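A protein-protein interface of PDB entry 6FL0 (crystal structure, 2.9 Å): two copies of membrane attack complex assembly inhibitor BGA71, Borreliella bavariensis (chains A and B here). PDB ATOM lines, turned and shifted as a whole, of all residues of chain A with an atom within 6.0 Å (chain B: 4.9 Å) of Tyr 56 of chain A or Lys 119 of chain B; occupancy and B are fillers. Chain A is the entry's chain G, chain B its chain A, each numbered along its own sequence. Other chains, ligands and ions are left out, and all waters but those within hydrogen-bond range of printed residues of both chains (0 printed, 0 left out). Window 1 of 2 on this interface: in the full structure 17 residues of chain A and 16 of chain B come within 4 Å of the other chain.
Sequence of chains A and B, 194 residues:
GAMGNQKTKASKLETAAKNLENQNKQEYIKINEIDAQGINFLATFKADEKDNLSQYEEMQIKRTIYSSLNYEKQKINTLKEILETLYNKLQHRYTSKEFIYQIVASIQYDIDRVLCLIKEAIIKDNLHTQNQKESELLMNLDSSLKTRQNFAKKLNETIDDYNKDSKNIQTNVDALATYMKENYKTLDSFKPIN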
ATOM      1  N   SER A  54      19.415  13.906   4.032  1.00  0.00           N
ATOM      2  CA  SER A  54      20.352  14.065   2.939  1.00  0.00           C
ATOM      3  C   SER A  54      19.879  13.240   1.729  1.00  0.00           C
ATOM      4  O   SER A  54      19.134  12.246   1.849  1.00  0.00           O
ATOM      5  CB  SER A  54      21.765  13.703   3.339  1.00  0.00           C
ATOM      6  OG  SER A  54      22.084  12.378   2.957  1.00  0.00           O
ATOM      7  N   GLN A  55      20.359  13.673   0.564  1.00  0.00           N
ATOM      8  CA  GLN A  55      19.995  13.134  -0.711  1.00  0.00           C
ATOM      9  C   GLN A  55      20.454  11.676  -0.728  1.00  0.00           C
ATOM     10  O   GLN A  55      19.739  10.797  -1.200  1.00  0.00           O
ATOM     11  CB  GLN A  55      20.643  13.974  -1.816  1.00  0.00           C
ATOM     12  CG  GLN A  55      20.526  15.488  -1.599  1.00  0.00           C
ATOM     13  CD  GLN A  55      21.450  16.035  -0.527  1.00  0.00           C
ATOM     14  OE1 GLN A  55      22.646  15.748  -0.499  1.00  0.00           O
ATOM     15  NE2 GLN A  55      20.905  16.830   0.386  1.00  0.00           N
ATOM     16  N   TYR A  56      21.643  11.448  -0.152  1.00  0.00           N
ATOM     17  CA  TYR A  56      22.268  10.140  -0.026  1.00  0.00           C
ATOM     18  C   TYR A  56      21.406   9.224   0.844  1.00  0.00           C
ATOM     19  O   TYR A  56      21.161   8.100   0.455  1.00  0.00           O
ATOM     20  CB  TYR A  56      23.683  10.254   0.558  1.00  0.00           C
ATOM     21  CG  TYR A  56      24.199   8.956   1.127  1.00  0.00           C
ATOM     22  CD1 TYR A  56      24.533   7.904   0.288  1.00  0.00           C
ATOM     23  CD2 TYR A  56      24.285   8.748   2.496  1.00  0.00           C
ATOM     24  CE1 TYR A  56      24.959   6.685   0.788  1.00  0.00           C
ATOM     25  CE2 TYR A  56      24.708   7.531   3.012  1.00  0.00           C
ATOM     26  CZ  TYR A  56      25.046   6.497   2.155  1.00  0.00           C
ATOM     27  OH  TYR A  56      25.472   5.295   2.639  1.00  0.00           O
ATOM     28  N   GLU A  57      20.990   9.719   2.017  1.00  0.00           N
ATOM     29  CA  GLU A  57      20.193   8.959   3.020  1.00  0.00           C
ATOM     30  C   GLU A  57      18.816   8.596   2.437  1.00  0.00           C
ATOM     31  O   GLU A  57      18.363   7.453   2.547  1.00  0.00           O
ATOM     32  CB  GLU A  57      19.977   9.767   4.307  1.00  0.00           C
ATOM     33  CG  GLU A  57      21.254  10.158   5.043  1.00  0.00           C
ATOM     34  CD  GLU A  57      21.031  10.988   6.299  1.00  0.00           C
ATOM     35  OE1 GLU A  57      20.870  12.223   6.196  1.00  0.00           O
ATOM     36  OE2 GLU A  57      21.002  10.388   7.385  1.00  0.00           O
ATOM     37  N   GLU A  58      18.154   9.590   1.832  1.00  0.00           N
ATOM     38  CA  GLU A  58      16.909   9.406   1.079  1.00  0.00           C
ATOM     39  C   GLU A  58      17.026   8.222   0.105  1.00  0.00           C
ATOM     40  O   GLU A  58      16.084   7.471  -0.110  1.00  0.00           O
ATOM     41  CB  GLU A  58      16.592  10.699   0.325  1.00  0.00           C
ATOM     42  CG  GLU A  58      15.583  10.538  -0.802  1.00  0.00           C
ATOM     43  CD  GLU A  58      15.127  11.849  -1.422  1.00  0.00           C
ATOM     44  OE1 GLU A  58      15.345  12.911  -0.782  1.00  0.00           O
ATOM     45  OE2 GLU A  58      14.564  11.815  -2.544  1.00  0.00           O
ATOM     46  N   MET A  59      18.193   8.085  -0.511  1.00  0.00           N
ATOM     47  CA  MET A  59      18.404   7.149  -1.558  1.00  0.00           C
ATOM     48  C   MET A  59      18.615   5.742  -0.978  1.00  0.00           C
ATOM     49  O   MET A  59      18.056   4.765  -1.472  1.00  0.00           O
ATOM     50  CB  MET A  59      19.616   7.604  -2.375  1.00  0.00           C
ATOM     51  CG  MET A  59      19.883   6.768  -3.603  1.00  0.00           C
ATOM     52  SD  MET A  59      18.456   6.643  -4.706  1.00  0.00           S
ATOM     53  CE  MET A  59      18.771   4.994  -5.328  1.00  0.00           C
ATOM     54  N   GLN A  60      19.417   5.636   0.084  1.00  0.00           N
ATOM     55  CA  GLN A  60      19.687   4.345   0.737  1.00  0.00           C
ATOM     56  C   GLN A  60      18.376   3.742   1.266  1.00  0.00           C
ATOM     57  O   GLN A  60      18.117   2.554   1.082  1.00  0.00           O
ATOM     58  CB  GLN A  60      20.710   4.504   1.866  1.00  0.00           C
ATOM     59  CG  GLN A  60      22.094   4.917   1.384  1.00  0.00           C
ATOM     60  CD  GLN A  60      22.597   4.051   0.250  1.00  0.00           C
ATOM     61  OE1 GLN A  60      22.511   4.419  -0.925  1.00  0.00           O
ATOM     62  NE2 GLN A  60      23.112   2.880   0.596  1.00  0.00           N
ATOM     63  N   ILE A  61      17.552   4.564   1.924  1.00  0.00           N
ATOM     64  CA  ILE A  61      16.270   4.101   2.454  1.00  0.00           C
ATOM     65  C   ILE A  61      15.488   3.426   1.315  1.00  0.00           C
ATOM     66  O   ILE A  61      15.012   2.291   1.453  1.00  0.00           O
ATOM     67  CB  ILE A  61      15.492   5.263   3.114  1.00  0.00           C
ATOM     68  CG1 ILE A  61      16.166   5.734   4.404  1.00  0.00           C
ATOM     69  CG2 ILE A  61      14.041   4.894   3.369  1.00  0.00           C
ATOM     70  CD1 ILE A  61      15.882   7.178   4.752  1.00  0.00           C
ATOM     71  N   TYR A 109      22.493  -0.014   5.171  1.00  0.00           N
ATOM     72  CA  TYR A 109      23.882   0.325   5.428  1.00  0.00           C
ATOM     73  C   TYR A 109      24.758  -0.934   5.526  1.00  0.00           C
ATOM     74  O   TYR A 109      25.847  -0.980   4.948  1.00  0.00           O
ATOM     75  CB  TYR A 109      24.043   1.142   6.714  1.00  0.00           C
ATOM     76  CG  TYR A 109      25.476   1.205   7.180  1.00  0.00           C
ATOM     77  CD1 TYR A 109      26.453   1.801   6.394  1.00  0.00           C
ATOM     78  CD2 TYR A 109      25.877   0.594   8.361  1.00  0.00           C
ATOM     79  CE1 TYR A 109      27.781   1.836   6.793  1.00  0.00           C
ATOM     80  CE2 TYR A 109      27.199   0.620   8.776  1.00  0.00           C
ATOM     81  CZ  TYR A 109      28.154   1.247   7.993  1.00  0.00           C
ATOM     82  OH  TYR A 109      29.459   1.273   8.402  1.00  0.00           O
ATOM     83  N   ASP A 112      25.948  -2.406   2.444  1.00  0.00           N
ATOM     84  CA  ASP A 112      26.935  -1.464   1.937  1.00  0.00           C
ATOM     85  C   ASP A 112      28.288  -1.677   2.633  1.00  0.00           C
ATOM     86  O   ASP A 112      29.322  -1.704   1.962  1.00  0.00           O
ATOM     87  CB  ASP A 112      26.480  -0.016   2.132  1.00  0.00           C
ATOM     88  CG  ASP A 112      25.342   0.404   1.229  1.00  0.00           C
ATOM     89  OD1 ASP A 112      24.595  -0.475   0.768  1.00  0.00           O
ATOM     90  OD2 ASP A 112      25.212   1.615   1.004  1.00  0.00           O
ATOM     91  N   ALA B  17      29.336  13.837   0.981  1.00  0.00           N
ATOM     92  CA  ALA B  17      28.783  12.599   0.423  1.00  0.00           C
ATOM     93  C   ALA B  17      28.026  12.868  -0.882  1.00  0.00           C
ATOM     94  O   ALA B  17      28.029  12.024  -1.777  1.00  0.00           O
ATOM     95  CB  ALA B  17      27.872  11.950   1.435  1.00  0.00           C
ATOM     96  N   GLU B  21      29.158  11.647  -4.614  1.00  0.00           N
ATOM     97  CA  GLU B  21      28.126  10.767  -5.184  1.00  0.00           C
ATOM     98  C   GLU B  21      27.849  11.175  -6.619  1.00  0.00           C
ATOM     99  O   GLU B  21      27.906  10.317  -7.471  1.00  0.00           O
ATOM    100  CB  GLU B  21      26.849  10.921  -4.373  1.00  0.00           C
ATOM    101  CG  GLU B  21      26.047   9.645  -4.268  1.00  0.00           C
ATOM    102  CD  GLU B  21      26.810   8.415  -3.821  1.00  0.00           C
ATOM    103  OE1 GLU B  21      27.812   8.063  -4.470  1.00  0.00           O
ATOM    104  OE2 GLU B  21      26.378   7.806  -2.844  1.00  0.00           O
ATOM    105  N   VAL B 114      37.307   6.726   2.074  1.00  0.00           N
ATOM    106  CA  VAL B 114      36.876   7.882   2.854  1.00  0.00           C
ATOM    107  C   VAL B 114      35.362   8.055   2.677  1.00  0.00           C
ATOM    108  O   VAL B 114      34.666   8.392   3.632  1.00  0.00           O
ATOM    109  CB  VAL B 114      37.640   9.169   2.482  1.00  0.00           C
ATOM    110  CG1 VAL B 114      37.054  10.389   3.166  1.00  0.00           C
ATOM    111  CG2 VAL B 114      39.120   9.065   2.809  1.00  0.00           C
ATOM    112  N   LEU B 115      34.853   7.821   1.464  1.00  0.00           N
ATOM    113  CA  LEU B 115      33.424   7.993   1.207  1.00  0.00           C
ATOM    114  C   LEU B 115      32.627   6.878   1.902  1.00  0.00           C
ATOM    115  O   LEU B 115      31.508   7.118   2.312  1.00  0.00           O
ATOM    116  CB  LEU B 115      33.159   8.018  -0.302  1.00  0.00           C
ATOM    117  CG  LEU B 115      31.686   8.112  -0.690  1.00  0.00           C
ATOM    118  CD1 LEU B 115      31.013   9.275   0.024  1.00  0.00           C
ATOM    119  CD2 LEU B 115      31.512   8.244  -2.192  1.00  0.00           C
ATOM    120  N   CYS B 116      33.200   5.671   2.021  1.00  0.00           N
ATOM    121  CA  CYS B 116      32.583   4.592   2.807  1.00  0.00           C
ATOM    122  C   CYS B 116      32.447   5.041   4.266  1.00  0.00           C
ATOM    123  O   CYS B 116      31.419   4.817   4.885  1.00  0.00           O
ATOM    124  CB  CYS B 116      33.387   3.294   2.789  1.00  0.00           C
ATOM    125  SG  CYS B 116      33.259   2.341   1.253  1.00  0.00           S
ATOM    126  N   LEU B 117      33.509   5.672   4.783  1.00  0.00           N
ATOM    127  CA  LEU B 117      33.612   6.126   6.183  1.00  0.00           C
ATOM    128  C   LEU B 117      32.732   7.359   6.437  1.00  0.00           C
ATOM    129  O   LEU B 117      32.120   7.480   7.492  1.00  0.00           O
ATOM    130  CB  LEU B 117      35.081   6.439   6.496  1.00  0.00           C
ATOM    131  CG  LEU B 117      36.026   5.238   6.522  1.00  0.00           C
ATOM    132  CD1 LEU B 117      37.467   5.695   6.661  1.00  0.00           C
ATOM    133  CD2 LEU B 117      35.676   4.264   7.637  1.00  0.00           C
ATOM    134  N   ILE B 118      32.719   8.285   5.475  1.00  0.00           N
ATOM    135  CA  ILE B 118      31.879   9.484   5.506  1.00  0.00           C
ATOM    136  C   ILE B 118      30.410   9.056   5.600  1.00  0.00           C
ATOM    137  O   ILE B 118      29.629   9.665   6.342  1.00  0.00           O
ATOM    138  CB  ILE B 118      32.136  10.360   4.259  1.00  0.00           C
ATOM    139  CG1 ILE B 118      33.584  10.860   4.201  1.00  0.00           C
ATOM    140  CG2 ILE B 118      31.124  11.497   4.164  1.00  0.00           C
ATOM    141  CD1 ILE B 118      33.792  12.264   4.684  1.00  0.00           C
ATOM    142  N   LYS B 119      30.053   8.019   4.832  1.00  0.00           N
ATOM    143  CA  LYS B 119      28.682   7.512   4.749  1.00  0.00           C
ATOM    144  C   LYS B 119      28.298   6.833   6.071  1.00  0.00           C
ATOM    145  O   LYS B 119      27.223   7.100   6.612  1.00  0.00           O
ATOM    146  CB  LYS B 119      28.520   6.554   3.565  1.00  0.00           C
ATOM    147  CG  LYS B 119      28.332   7.232   2.215  1.00  0.00           C
ATOM    148  CD  LYS B 119      28.383   6.263   1.054  1.00  0.00           C
ATOM    149  CE  LYS B 119      28.377   6.954  -0.293  1.00  0.00           C
ATOM    150  NZ  LYS B 119      28.093   6.002  -1.391  1.00  0.00           N
ATOM    151  N   GLU B 120      29.186   5.976   6.586  1.00  0.00           N
ATOM    152  CA  GLU B 120      28.983   5.298   7.873  1.00  0.00           C
ATOM    153  C   GLU B 120      28.646   6.314   8.975  1.00  0.00           C
ATOM    154  O   GLU B 120      27.707   6.109   9.742  1.00  0.00           O
ATOM    155  CB  GLU B 120      30.244   4.515   8.234  1.00  0.00           C
ATOM    156  CG  GLU B 120      30.310   4.080   9.684  1.00  0.00           C
ATOM    157  CD  GLU B 120      31.657   3.493  10.053  1.00  0.00           C
ATOM    158  OE1 GLU B 120      32.529   3.438   9.170  1.00  0.00           O
ATOM    159  OE2 GLU B 120      31.835   3.110  11.218  1.00  0.00           O
ATOM    160  N   ALA B 121      29.437   7.393   9.043  1.00  0.00           N
ATOM    161  CA  ALA B 121      29.315   8.441  10.051  1.00  0.00           C
ATOM    162  C   ALA B 121      27.958   9.145   9.928  1.00  0.00           C
ATOM    163  O   ALA B 121      27.364   9.569  10.922  1.00  0.00           O
ATOM    164  CB  ALA B 121      30.451   9.422   9.895  1.00  0.00           C
ATOM    165  N   ILE B 122      27.483   9.284   8.690  1.00  0.00           N
ATOM    166  CA  ILE B 122      26.232   9.960   8.427  1.00  0.00           C
ATOM    167  C   ILE B 122      25.085   9.091   8.956  1.00  0.00           C
ATOM    168  O   ILE B 122      24.178   9.597   9.611  1.00  0.00           O
ATOM    169  CB  ILE B 122      26.101  10.300   6.927  1.00  0.00           C
ATOM    170  CG1 ILE B 122      26.936  11.536   6.569  1.00  0.00           C
ATOM    171  CG2 ILE B 122      24.642  10.468   6.515  1.00  0.00           C
ATOM    172  CD1 ILE B 122      27.327  11.620   5.109  1.00  0.00           C
ATOM    173  N   ILE B 123      25.151   7.784   8.684  1.00  0.00           N
ATOM    174  CA  ILE B 123      24.097   6.859   9.036  1.00  0.00           C
ATOM    175  C   ILE B 123      24.098   6.685  10.555  1.00  0.00           C
ATOM    176  O   ILE B 123      23.057   6.867  11.184  1.00  0.00           O
ATOM    177  CB  ILE B 123      24.258   5.527   8.275  1.00  0.00           C
ATOM    178  CG1 ILE B 123      24.068   5.719   6.763  1.00  0.00           C
ATOM    179  CG2 ILE B 123      23.329   4.449   8.833  1.00  0.00           C
ATOM    180  CD1 ILE B 123      22.684   6.189   6.348  1.00  0.00           C
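Of the 12 printed residues of chain B, 5 touch a printed residue of chain A. Hydrophobic or aromatic side chains of chain B that line the printed part of chain A: Ile 122 and Ile 123. Of the 10 printed residues of chain A, 3 touch a printed residue of chain B. Hydrophobic or aromatic side chains of chain A within 4 Å of the printed part of chain B: Tyr 56 and Tyr 109. Along chain A the printed residues that touch a printed residue of chain B span positions 56 to 109. Among the printed residues, 5 pairs touch across the chains. Among the printed residues, no Asp or Glu carboxylate lies within 4 Å of a Lys or Arg side-chain nitrogen of the other chain.
Among the printed residues, pairs that only touch across the chains: Tyr 109 of chain A with Glu 120 of chain B (3.2 Å), Tyr 56 of chain A with Lys 119 of chain B (3.4 Å), Tyr 56 of chain A with Glu 21 of chain B (3.6 Å), Glu 57 of chain A with Ile 122 of chain B (3.7 Å) and Tyr 109 of chain A with Ile 123 of chain B (3.99 Å).
The side-chain hydroxyl of Ser 54 of chain A lies within hydrogen-bond range of the backbone NH of Glu 57 of chain A. OE2 of Glu 21 of chain B is in salt-bridge range of NZ of Lys 119 of chain B (2.9 Å). The backbone NH (N) of Tyr 56 of chain A sits close to the side-chain hydroxyl (OG) of Ser 54 of chain A, at 3.3 Å.
No position is printed for both chains. Of the 5 pairs that touch across the chains among the printed residues, none has its exchanged pair printed and touching as well.
Tyr 56 of chain A touches just these residues of chain B: Glu 21 (3.6 Å) and Lys 119 (3.4 Å). Printed residues of chain A within 4 Å of Lys 119 of chain B: Tyr 56. Printed residues of chain A within 4 Å of Ile 123 of chain B: Tyr 109 (3.99 Å). Of the printed residues of chain A, Ile 122 of chain B touches Glu 57 (3.7 Å). Printed residues of chain A within 4 Å of Glu 21 of chain B: Tyr 56 (3.6 Å). Printed residues of chain A within 4 Å of Glu 120 of chain B: Tyr 109. Asp 112 of chain A touches none of the printed residues of chain B. Glu 58 of chain A touches none of the printed residues of chain B. The nearest residue of chain B that does not touch Tyr 56 of chain A is Ile 123 of chain B (4.1 Å). The nearest residue of chain A that does not touch Lys 119 of chain B is Tyr 109 of chain A (5.1 Å). The nearest printed residue of chain A that does not touch Glu 120 of chain B is Tyr 56 of chain A (5.5 Å).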
